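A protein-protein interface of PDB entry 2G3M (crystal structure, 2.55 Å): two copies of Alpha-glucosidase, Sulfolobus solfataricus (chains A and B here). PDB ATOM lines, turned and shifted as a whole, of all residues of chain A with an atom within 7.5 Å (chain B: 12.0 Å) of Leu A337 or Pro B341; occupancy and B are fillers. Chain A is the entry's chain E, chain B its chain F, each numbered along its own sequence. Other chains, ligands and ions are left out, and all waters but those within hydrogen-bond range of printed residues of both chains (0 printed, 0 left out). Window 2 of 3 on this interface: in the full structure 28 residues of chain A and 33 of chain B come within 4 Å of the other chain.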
ATOM      1  N   ILE A 331     -31.021 -17.840 -11.489  1.00  0.00           N
ATOM      2  CA  ILE A 331     -31.291 -17.744 -10.068  1.00  0.00           C
ATOM      3  C   ILE A 331     -30.931 -19.053  -9.379  1.00  0.00           C
ATOM      4  O   ILE A 331     -30.519 -19.068  -8.221  1.00  0.00           O
ATOM      5  CB  ILE A 331     -32.768 -17.400  -9.841  1.00  0.00           C
ATOM      6  CG1 ILE A 331     -33.004 -15.951 -10.282  1.00  0.00           C
ATOM      7  CG2 ILE A 331     -33.152 -17.632  -8.380  1.00  0.00           C
ATOM      8  CD1 ILE A 331     -34.453 -15.586 -10.483  1.00  0.00           C
ATOM      9  N   GLU A 332     -31.069 -20.150 -10.107  1.00  0.00           N
ATOM     10  CA  GLU A 332     -30.750 -21.461  -9.571  1.00  0.00           C
ATOM     11  C   GLU A 332     -29.245 -21.525  -9.282  1.00  0.00           C
ATOM     12  O   GLU A 332     -28.821 -21.981  -8.220  1.00  0.00           O
ATOM     13  CB  GLU A 332     -31.149 -22.516 -10.590  1.00  0.00           C
ATOM     14  CG  GLU A 332     -31.291 -23.908 -10.052  1.00  0.00           C
ATOM     15  CD  GLU A 332     -32.086 -24.788 -11.003  1.00  0.00           C
ATOM     16  OE1 GLU A 332     -33.268 -24.457 -11.259  1.00  0.00           O
ATOM     17  OE2 GLU A 332     -31.534 -25.799 -11.496  1.00  0.00           O
ATOM     18  N   ILE A 333     -28.447 -21.056 -10.236  1.00  0.00           N
ATOM     19  CA  ILE A 333     -27.001 -21.044 -10.088  1.00  0.00           C
ATOM     20  C   ILE A 333     -26.578 -20.187  -8.889  1.00  0.00           C
ATOM     21  O   ILE A 333     -25.677 -20.568  -8.145  1.00  0.00           O
ATOM     22  CB  ILE A 333     -26.326 -20.522 -11.385  1.00  0.00           C
ATOM     23  CG1 ILE A 333     -26.564 -21.526 -12.519  1.00  0.00           C
ATOM     24  CG2 ILE A 333     -24.828 -20.298 -11.158  1.00  0.00           C
ATOM     25  CD1 ILE A 333     -26.052 -21.071 -13.874  1.00  0.00           C
ATOM     26  N   ARG A 334     -27.233 -19.041  -8.705  1.00  0.00           N
ATOM     27  CA  ARG A 334     -26.931 -18.148  -7.584  1.00  0.00           C
ATOM     28  C   ARG A 334     -27.310 -18.775  -6.237  1.00  0.00           C
ATOM     29  O   ARG A 334     -26.614 -18.588  -5.245  1.00  0.00           O
ATOM     30  CB  ARG A 334     -27.661 -16.813  -7.750  1.00  0.00           C
ATOM     31  CG  ARG A 334     -27.203 -15.996  -8.953  1.00  0.00           C
ATOM     32  CD  ARG A 334     -28.163 -14.839  -9.245  1.00  0.00           C
ATOM     33  NE  ARG A 334     -27.963 -14.291 -10.591  1.00  0.00           N
ATOM     34  CZ  ARG A 334     -28.823 -13.485 -11.218  1.00  0.00           C
ATOM     35  NH1 ARG A 334     -29.958 -13.121 -10.629  1.00  0.00           N
ATOM     36  NH2 ARG A 334     -28.550 -13.047 -12.440  1.00  0.00           N
ATOM     37  N   ASP A 335     -28.414 -19.512  -6.194  1.00  0.00           N
ATOM     38  CA  ASP A 335     -28.824 -20.156  -4.952  1.00  0.00           C
ATOM     39  C   ASP A 335     -27.768 -21.154  -4.493  1.00  0.00           C
ATOM     40  O   ASP A 335     -27.339 -21.138  -3.344  1.00  0.00           O
ATOM     41  CB  ASP A 335     -30.148 -20.910  -5.122  1.00  0.00           C
ATOM     42  CG  ASP A 335     -31.345 -19.986  -5.243  1.00  0.00           C
ATOM     43  OD1 ASP A 335     -31.209 -18.787  -4.912  1.00  0.00           O
ATOM     44  OD2 ASP A 335     -32.424 -20.471  -5.657  1.00  0.00           O
ATOM     45  N   VAL A 336     -27.354 -22.025  -5.404  1.00  0.00           N
ATOM     46  CA  VAL A 336     -26.377 -23.049  -5.087  1.00  0.00           C
ATOM     47  C   VAL A 336     -24.954 -22.560  -4.823  1.00  0.00           C
ATOM     48  O   VAL A 336     -24.299 -23.046  -3.907  1.00  0.00           O
ATOM     49  CB  VAL A 336     -26.336 -24.113  -6.200  1.00  0.00           C
ATOM     50  CG1 VAL A 336     -25.289 -25.168  -5.879  1.00  0.00           C
ATOM     51  CG2 VAL A 336     -27.704 -24.751  -6.344  1.00  0.00           C
ATOM     52  N   LEU A 337     -24.476 -21.606  -5.613  1.00  0.00           N
ATOM     53  CA  LEU A 337     -23.113 -21.105  -5.454  1.00  0.00           C
ATOM     54  C   LEU A 337     -23.069 -19.705  -4.854  1.00  0.00           C
ATOM     55  O   LEU A 337     -22.126 -18.951  -5.077  1.00  0.00           O
ATOM     56  CB  LEU A 337     -22.415 -21.110  -6.813  1.00  0.00           C
ATOM     57  CG  LEU A 337     -22.538 -22.435  -7.572  1.00  0.00           C
ATOM     58  CD1 LEU A 337     -21.938 -22.301  -8.968  1.00  0.00           C
ATOM     59  CD2 LEU A 337     -21.844 -23.533  -6.789  1.00  0.00           C
ATOM     60  N   SER A 338     -24.096 -19.380  -4.077  1.00  0.00           N
ATOM     61  CA  SER A 338     -24.238 -18.075  -3.432  1.00  0.00           C
ATOM     62  C   SER A 338     -23.023 -17.552  -2.660  1.00  0.00           C
ATOM     63  O   SER A 338     -22.329 -16.637  -3.113  1.00  0.00           O
ATOM     64  CB  SER A 338     -25.454 -18.105  -2.492  1.00  0.00           C
ATOM     65  OG  SER A 338     -25.604 -16.880  -1.788  1.00  0.00           O
ATOM     66  N   SER A 339     -22.779 -18.131  -1.488  1.00  0.00           N
ATOM     67  CA  SER A 339     -21.683 -17.699  -0.631  1.00  0.00           C
ATOM     68  C   SER A 339     -20.286 -18.142  -1.076  1.00  0.00           C
ATOM     69  O   SER A 339     -19.355 -18.177  -0.267  1.00  0.00           O
ATOM     70  CB  SER A 339     -21.943 -18.166   0.806  1.00  0.00           C
ATOM     71  OG  SER A 339     -21.065 -17.531   1.725  1.00  0.00           O
ATOM     72  N   LEU A 340     -20.132 -18.476  -2.351  1.00  0.00           N
ATOM     73  CA  LEU A 340     -18.825 -18.889  -2.847  1.00  0.00           C
ATOM     74  C   LEU A 340     -18.138 -17.676  -3.474  1.00  0.00           C
ATOM     75  O   LEU A 340     -18.609 -17.132  -4.473  1.00  0.00           O
ATOM     76  CB  LEU A 340     -18.968 -20.008  -3.872  1.00  0.00           C
ATOM     77  CG  LEU A 340     -17.730 -20.894  -3.979  1.00  0.00           C
ATOM     78  CD1 LEU A 340     -17.426 -21.508  -2.618  1.00  0.00           C
ATOM     79  CD2 LEU A 340     -17.962 -21.977  -5.014  1.00  0.00           C
ATOM     80  N   PRO A 341     -17.005 -17.246  -2.887  1.00  0.00           N
ATOM     81  CA  PRO A 341     -16.181 -16.103  -3.300  1.00  0.00           C
ATOM     82  C   PRO A 341     -15.680 -16.151  -4.738  1.00  0.00           C
ATOM     83  O   PRO A 341     -14.596 -15.656  -5.046  1.00  0.00           O
ATOM     84  CB  PRO A 341     -15.035 -16.137  -2.298  1.00  0.00           C
ATOM     85  CG  PRO A 341     -14.867 -17.602  -2.057  1.00  0.00           C
ATOM     86  CD  PRO A 341     -16.294 -18.048  -1.875  1.00  0.00           C
ATOM     87  N   VAL A 342     -16.480 -16.731  -5.620  1.00  0.00           N
ATOM     88  CA  VAL A 342     -16.101 -16.857  -7.014  1.00  0.00           C
ATOM     89  C   VAL A 342     -16.930 -15.972  -7.936  1.00  0.00           C
ATOM     90  O   VAL A 342     -18.007 -15.505  -7.575  1.00  0.00           O
ATOM     91  CB  VAL A 342     -16.215 -18.329  -7.462  1.00  0.00           C
ATOM     92  CG1 VAL A 342     -16.041 -18.441  -8.950  1.00  0.00           C
ATOM     93  CG2 VAL A 342     -15.157 -19.163  -6.753  1.00  0.00           C
ATOM     94  N   GLN A 343     -16.397 -15.739  -9.130  1.00  0.00           N
ATOM     95  CA  GLN A 343     -17.049 -14.925 -10.144  1.00  0.00           C
ATOM     96  C   GLN A 343     -17.704 -15.852 -11.169  1.00  0.00           C
ATOM     97  O   GLN A 343     -17.040 -16.730 -11.727  1.00  0.00           O
ATOM     98  CB  GLN A 343     -16.001 -14.036 -10.817  1.00  0.00           C
ATOM     99  CG  GLN A 343     -16.516 -13.151 -11.929  1.00  0.00           C
ATOM    100  CD  GLN A 343     -15.435 -12.235 -12.471  1.00  0.00           C
ATOM    101  OE1 GLN A 343     -15.632 -11.540 -13.468  1.00  0.00           O
ATOM    102  NE2 GLN A 343     -14.281 -12.226 -11.810  1.00  0.00           N
ATOM    103  N   PHE A 344     -19.004 -15.668 -11.405  1.00  0.00           N
ATOM    104  CA  PHE A 344     -19.734 -16.499 -12.363  1.00  0.00           C
ATOM    105  C   PHE A 344     -19.525 -16.002 -13.787  1.00  0.00           C
ATOM    106  O   PHE A 344     -19.483 -14.797 -14.026  1.00  0.00           O
ATOM    107  CB  PHE A 344     -21.240 -16.490 -12.066  1.00  0.00           C
ATOM    108  CG  PHE A 344     -21.594 -16.829 -10.641  1.00  0.00           C
ATOM    109  CD1 PHE A 344     -20.912 -17.827  -9.952  1.00  0.00           C
ATOM    110  CD2 PHE A 344     -22.637 -16.166  -9.999  1.00  0.00           C
ATOM    111  CE1 PHE A 344     -21.263 -18.159  -8.642  1.00  0.00           C
ATOM    112  CE2 PHE A 344     -22.997 -16.489  -8.690  1.00  0.00           C
ATOM    113  CZ  PHE A 344     -22.308 -17.487  -8.011  1.00  0.00           C
ATOM    114  N   ARG A 345     -19.384 -16.924 -14.736  1.00  0.00           N
ATOM    115  CA  ARG A 345     -19.211 -16.519 -16.126  1.00  0.00           C
ATOM    116  C   ARG A 345     -20.582 -16.056 -16.571  1.00  0.00           C
ATOM    117  O   ARG A 345     -21.592 -16.670 -16.232  1.00  0.00           O
ATOM    118  CB  ARG A 345     -18.724 -17.688 -16.993  1.00  0.00           C
ATOM    119  CG  ARG A 345     -19.687 -18.859 -17.104  1.00  0.00           C
ATOM    120  CD  ARG A 345     -18.989 -20.089 -17.682  1.00  0.00           C
ATOM    121  NE  ARG A 345     -19.884 -21.242 -17.765  1.00  0.00           N
ATOM    122  CZ  ARG A 345     -19.482 -22.496 -17.961  1.00  0.00           C
ATOM    123  NH1 ARG A 345     -18.190 -22.770 -18.096  1.00  0.00           N
ATOM    124  NH2 ARG A 345     -20.376 -23.477 -18.024  1.00  0.00           N
ATOM    125  N   ASP A 346     -20.621 -14.959 -17.312  1.00  0.00           N
ATOM    126  CA  ASP A 346     -21.885 -14.407 -17.776  1.00  0.00           C
ATOM    127  C   ASP A 346     -22.297 -15.032 -19.109  1.00  0.00           C
ATOM    128  O   ASP A 346     -21.935 -14.543 -20.180  1.00  0.00           O
ATOM    129  CB  ASP A 346     -21.756 -12.880 -17.900  1.00  0.00           C
ATOM    130  CG  ASP A 346     -23.102 -12.172 -17.957  1.00  0.00           C
ATOM    131  OD1 ASP A 346     -24.005 -12.532 -17.172  1.00  0.00           O
ATOM    132  OD2 ASP A 346     -23.248 -11.241 -18.779  1.00  0.00           O
ATOM    133  N   ASP A 347     -23.037 -16.135 -19.034  1.00  0.00           N
ATOM    134  CA  ASP A 347     -23.512 -16.810 -20.231  1.00  0.00           C
ATOM    135  C   ASP A 347     -24.961 -16.392 -20.433  1.00  0.00           C
ATOM    136  O   ASP A 347     -25.860 -16.837 -19.719  1.00  0.00           O
ATOM    137  CB  ASP A 347     -23.411 -18.330 -20.078  1.00  0.00           C
ATOM    138  CG  ASP A 347     -23.932 -19.078 -21.300  1.00  0.00           C
ATOM    139  OD1 ASP A 347     -23.832 -18.537 -22.432  1.00  0.00           O
ATOM    140  OD2 ASP A 347     -24.431 -20.214 -21.133  1.00  0.00           O
ATOM    141  N   VAL A 350     -28.154 -18.638 -20.812  1.00  0.00           N
ATOM    142  CA  VAL A 350     -28.788 -19.199 -19.633  1.00  0.00           C
ATOM    143  C   VAL A 350     -30.142 -18.536 -19.358  1.00  0.00           C
ATOM    144  O   VAL A 350     -30.968 -19.096 -18.629  1.00  0.00           O
ATOM    145  CB  VAL A 350     -27.857 -19.087 -18.377  1.00  0.00           C
ATOM    146  CG1 VAL A 350     -27.872 -17.671 -17.809  1.00  0.00           C
ATOM    147  CG2 VAL A 350     -28.292 -20.079 -17.325  1.00  0.00           C
ATOM    148  N   ILE B 333      -8.010 -28.551 -17.701  1.00  0.00           N
ATOM    149  CA  ILE B 333      -8.813 -27.780 -16.770  1.00  0.00           C
ATOM    150  C   ILE B 333     -10.217 -27.636 -17.341  1.00  0.00           C
ATOM    151  O   ILE B 333     -11.216 -27.820 -16.643  1.00  0.00           O
ATOM    152  CB  ILE B 333      -8.210 -26.373 -16.557  1.00  0.00           C
ATOM    153  CG1 ILE B 333      -6.826 -26.495 -15.905  1.00  0.00           C
ATOM    154  CG2 ILE B 333      -9.154 -25.518 -15.714  1.00  0.00           C
ATOM    155  CD1 ILE B 333      -6.094 -25.175 -15.735  1.00  0.00           C
ATOM    156  N   ARG B 334     -10.278 -27.315 -18.624  1.00  0.00           N
ATOM    157  CA  ARG B 334     -11.538 -27.133 -19.322  1.00  0.00           C
ATOM    158  C   ARG B 334     -12.390 -28.408 -19.297  1.00  0.00           C
ATOM    159  O   ARG B 334     -13.594 -28.336 -19.103  1.00  0.00           O
ATOM    160  CB  ARG B 334     -11.253 -26.712 -20.763  1.00  0.00           C
ATOM    161  CG  ARG B 334     -12.394 -26.014 -21.469  1.00  0.00           C
ATOM    162  CD  ARG B 334     -11.986 -25.669 -22.899  1.00  0.00           C
ATOM    163  NE  ARG B 334     -10.669 -25.032 -22.941  1.00  0.00           N
ATOM    164  CZ  ARG B 334     -10.049 -24.656 -24.056  1.00  0.00           C
ATOM    165  NH1 ARG B 334     -10.631 -24.848 -25.238  1.00  0.00           N
ATOM    166  NH2 ARG B 334      -8.841 -24.097 -23.990  1.00  0.00           N
ATOM    167  N   ASP B 335     -11.773 -29.571 -19.486  1.00  0.00           N
ATOM    168  CA  ASP B 335     -12.519 -30.833 -19.476  1.00  0.00           C
ATOM    169  C   ASP B 335     -13.125 -31.173 -18.117  1.00  0.00           C
ATOM    170  O   ASP B 335     -14.220 -31.728 -18.044  1.00  0.00           O
ATOM    171  CB  ASP B 335     -11.633 -32.015 -19.898  1.00  0.00           C
ATOM    172  CG  ASP B 335     -11.318 -32.020 -21.384  1.00  0.00           C
ATOM    173  OD1 ASP B 335     -11.993 -31.295 -22.153  1.00  0.00           O
ATOM    174  OD2 ASP B 335     -10.393 -32.769 -21.780  1.00  0.00           O
ATOM    175  N   VAL B 336     -12.408 -30.857 -17.044  1.00  0.00           N
ATOM    176  CA  VAL B 336     -12.889 -31.163 -15.707  1.00  0.00           C
ATOM    177  C   VAL B 336     -13.887 -30.151 -15.137  1.00  0.00           C
ATOM    178  O   VAL B 336     -14.866 -30.544 -14.510  1.00  0.00           O
ATOM    179  CB  VAL B 336     -11.704 -31.330 -14.729  1.00  0.00           C
ATOM    180  CG1 VAL B 336     -12.208 -31.512 -13.311  1.00  0.00           C
ATOM    181  CG2 VAL B 336     -10.865 -32.522 -15.138  1.00  0.00           C
ATOM    182  N   LEU B 337     -13.659 -28.860 -15.359  1.00  0.00           N
ATOM    183  CA  LEU B 337     -14.559 -27.836 -14.831  1.00  0.00           C
ATOM    184  C   LEU B 337     -15.399 -27.131 -15.899  1.00  0.00           C
ATOM    185  O   LEU B 337     -15.810 -25.983 -15.720  1.00  0.00           O
ATOM    186  CB  LEU B 337     -13.756 -26.791 -14.051  1.00  0.00           C
ATOM    187  CG  LEU B 337     -12.782 -27.339 -13.006  1.00  0.00           C
ATOM    188  CD1 LEU B 337     -12.107 -26.187 -12.290  1.00  0.00           C
ATOM    189  CD2 LEU B 337     -13.521 -28.223 -12.013  1.00  0.00           C
ATOM    190  N   SER B 338     -15.655 -27.816 -17.008  1.00  0.00           N
ATOM    191  CA  SER B 338     -16.444 -27.250 -18.101  1.00  0.00           C
ATOM    192  C   SER B 338     -17.880 -26.989 -17.668  1.00  0.00           C
ATOM    193  O   SER B 338     -18.508 -26.018 -18.096  1.00  0.00           O
ATOM    194  CB  SER B 338     -16.458 -28.213 -19.285  1.00  0.00           C
ATOM    195  OG  SER B 338     -16.880 -29.504 -18.867  1.00  0.00           O
ATOM    196  N   SER B 339     -18.392 -27.873 -16.816  1.00  0.00           N
ATOM    197  CA  SER B 339     -19.757 -27.766 -16.323  1.00  0.00           C
ATOM    198  C   SER B 339     -19.976 -26.517 -15.479  1.00  0.00           C
ATOM    199  O   SER B 339     -20.919 -25.766 -15.715  1.00  0.00           O
ATOM    200  CB  SER B 339     -20.125 -29.022 -15.516  1.00  0.00           C
ATOM    201  OG  SER B 339     -19.213 -29.264 -14.454  1.00  0.00           O
ATOM    202  N   LEU B 340     -19.104 -26.293 -14.503  1.00  0.00           N
ATOM    203  CA  LEU B 340     -19.225 -25.136 -13.623  1.00  0.00           C
ATOM    204  C   LEU B 340     -19.433 -23.813 -14.341  1.00  0.00           C
ATOM    205  O   LEU B 340     -18.637 -23.422 -15.194  1.00  0.00           O
ATOM    206  CB  LEU B 340     -18.001 -25.021 -12.718  1.00  0.00           C
ATOM    207  CG  LEU B 340     -18.160 -25.647 -11.334  1.00  0.00           C
ATOM    208  CD1 LEU B 340     -18.537 -27.120 -11.470  1.00  0.00           C
ATOM    209  CD2 LEU B 340     -16.864 -25.478 -10.553  1.00  0.00           C
ATOM    210  N   PRO B 341     -20.515 -23.100 -13.990  1.00  0.00           N
ATOM    211  CA  PRO B 341     -20.873 -21.803 -14.569  1.00  0.00           C
ATOM    212  C   PRO B 341     -19.960 -20.735 -13.974  1.00  0.00           C
ATOM    213  O   PRO B 341     -20.390 -19.628 -13.650  1.00  0.00           O
ATOM    214  CB  PRO B 341     -22.317 -21.635 -14.132  1.00  0.00           C
ATOM    215  CG  PRO B 341     -22.297 -22.238 -12.761  1.00  0.00           C
ATOM    216  CD  PRO B 341     -21.503 -23.508 -12.972  1.00  0.00           C
ATOM    217  N   VAL B 342     -18.689 -21.094 -13.836  1.00  0.00           N
ATOM    218  CA  VAL B 342     -17.681 -20.224 -13.258  1.00  0.00           C
ATOM    219  C   VAL B 342     -16.752 -19.645 -14.323  1.00  0.00           C
ATOM    220  O   VAL B 342     -16.699 -20.138 -15.448  1.00  0.00           O
ATOM    221  CB  VAL B 342     -16.840 -21.008 -12.223  1.00  0.00           C
ATOM    222  CG1 VAL B 342     -16.103 -22.150 -12.909  1.00  0.00           C
ATOM    223  CG2 VAL B 342     -15.859 -20.090 -11.545  1.00  0.00           C
ATOM    224  N   GLN B 343     -16.025 -18.595 -13.958  1.00  0.00           N
ATOM    225  CA  GLN B 343     -15.095 -17.953 -14.875  1.00  0.00           C
ATOM    226  C   GLN B 343     -13.660 -18.301 -14.497  1.00  0.00           C
ATOM    227  O   GLN B 343     -13.177 -17.901 -13.438  1.00  0.00           O
ATOM    228  CB  GLN B 343     -15.292 -16.437 -14.840  1.00  0.00           C
ATOM    229  CG  GLN B 343     -14.428 -15.687 -15.836  1.00  0.00           C
ATOM    230  CD  GLN B 343     -14.861 -14.244 -16.017  1.00  0.00           C
ATOM    231  OE1 GLN B 343     -14.249 -13.492 -16.779  1.00  0.00           O
ATOM    232  NE2 GLN B 343     -15.924 -13.849 -15.321  1.00  0.00           N
ATOM    233  N   PHE B 344     -12.986 -19.048 -15.366  1.00  0.00           N
ATOM    234  CA  PHE B 344     -11.609 -19.451 -15.110  1.00  0.00           C
ATOM    235  C   PHE B 344     -10.686 -18.247 -15.166  1.00  0.00           C
ATOM    236  O   PHE B 344     -10.969 -17.276 -15.864  1.00  0.00           O
ATOM    237  CB  PHE B 344     -11.129 -20.471 -16.149  1.00  0.00           C
ATOM    238  CG  PHE B 344     -12.051 -21.648 -16.337  1.00  0.00           C
ATOM    239  CD1 PHE B 344     -12.676 -22.252 -15.249  1.00  0.00           C
ATOM    240  CD2 PHE B 344     -12.267 -22.175 -17.611  1.00  0.00           C
ATOM    241  CE1 PHE B 344     -13.505 -23.362 -15.428  1.00  0.00           C
ATOM    242  CE2 PHE B 344     -13.089 -23.282 -17.802  1.00  0.00           C
ATOM    243  CZ  PHE B 344     -13.709 -23.878 -16.709  1.00  0.00           C
ATOM    244  N   ARG B 345      -9.587 -18.302 -14.423  1.00  0.00           N
ATOM    245  CA  ARG B 345      -8.624 -17.213 -14.457  1.00  0.00           C
ATOM    246  C   ARG B 345      -7.670 -17.620 -15.564  1.00  0.00           C
ATOM    247  O   ARG B 345      -7.275 -18.785 -15.656  1.00  0.00           O
ATOM    248  CB  ARG B 345      -7.859 -17.083 -13.134  1.00  0.00           C
ATOM    249  CG  ARG B 345      -6.936 -18.256 -12.819  1.00  0.00           C
ATOM    250  CD  ARG B 345      -5.937 -17.919 -11.712  1.00  0.00           C
ATOM    251  NE  ARG B 345      -5.052 -19.050 -11.428  1.00  0.00           N
ATOM    252  CZ  ARG B 345      -5.410 -20.130 -10.737  1.00  0.00           C
ATOM    253  NH1 ARG B 345      -6.639 -20.226 -10.248  1.00  0.00           N
ATOM    254  NH2 ARG B 345      -4.544 -21.121 -10.544  1.00  0.00           N
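Of the 13 printed residues of chain B, 6 touch a printed residue of chain A.
Printed residues of chain B that touch a printed residue of chain A: Ser B338, Ser B339, Leu B340, Pro B341, Val B342 and Gln B343.
Hydrophobic or aromatic side chains of chain B within 4 Å of the printed part of chain A: Pro B341 and Val B342.
Of the 18 printed residues of chain A, 6 touch a printed residue of chain B.
Hydrophobic or aromatic side chains of chain A that line the printed part of chain B: Ile A333, Leu A337, Val A342 and Phe A344.
Among the printed residues, no Asp or Glu carboxylate lies within 4 Å of a Lys or Arg side-chain nitrogen of the other chain.
The side-chain amide oxygen of Gln A343 lies within hydrogen-bond range of the side-chain amide nitrogen of Gln B343 (3.0 Å).
O of Ser B338 lies within hydrogen-bond range of NH2 of Arg A345 (3.2 Å).
The backbone carbonyl oxygen of Ser B339 sits at hydrogen-bond distance from the guanidinium group of Arg A345 (3.3 Å).
The backbone carbonyl oxygen (O) of Leu B340 is in hydrogen-bond range of the guanidinium group (NH1) of Arg A345, at 3.0 Å.
The backbone carbonyl oxygen of Pro B341 is in hydrogen-bond range of the backbone NH of Arg A345 (3.1 Å).
Ile A333 touches Pro B341 (CG2 to CG, 3.6 Å).
Leu A337 touches Pro B341 (CD1 to CG, 3.8 Å).
CG1 of Val A342 touches CG2 of Val B342, 3.1 Å away.
O of Gln A343 touches CG2 of Val B342, 3.6 Å away.
Pro B341 touches Phe A344 (O to CA, 3.4 Å).
Gln B343 touches Phe A344 (NE2 to O, 3.9 Å).
Arg A345 touches Val B342 (CD to O, 3.2 Å).
Gln B343 touches Arg A345 (N to N, 3.8 Å).
Pro B341 touches four residues of chain A.
No residue of chain B comes within 4 Å of Val A336.
Ser A338 touches none of the printed residues of chain B.
No residue of chain B comes within 4 Å of Ser A339.
Leu A340 touches none of the printed residues of chain B.
Of chain B, only Val B342 comes within 4 Å of Val A342.
Arg A345 touches six residues of chain B.
Of the printed residues of chain A, Val B342 touches Val A342, Gln A343 and Arg A345.
Of the printed residues of chain A, Gln B343 touches Gln A343 (3.0 Å), Phe A344 (3.9 Å) and Arg A345 (3.8 Å).
Phe B344 touches none of the printed residues of chain A.
The nearest residue of chain A that does not touch Pro B341 is Gln A343 (4.8 Å).
The nearest printed residue of chain A that does not touch Leu B340 is Leu A337 (5.6 Å).
Leu A337 touches Pro B341, but with the chains exchanged Pro A341 does not touch Leu B337 (13.0 Å).
Val A342 touches its own counterpart, Val B342.
Phe A344 touches Gln B343, but with the chains exchanged Gln A343 does not touch Phe B344 (5.9 Å).
Arg A345 touches Ser B339, but with the chains exchanged Ser A339 does not touch Arg B345 (16.3 Å).
Of the 13 pairs that touch across the chains among the printed residues, 2 have their exchanged pair printed and touching as well.
The backbone carbonyl oxygen (O) of Arg B334 lies close to the side-chain hydroxyl (OG) of Ser B338.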
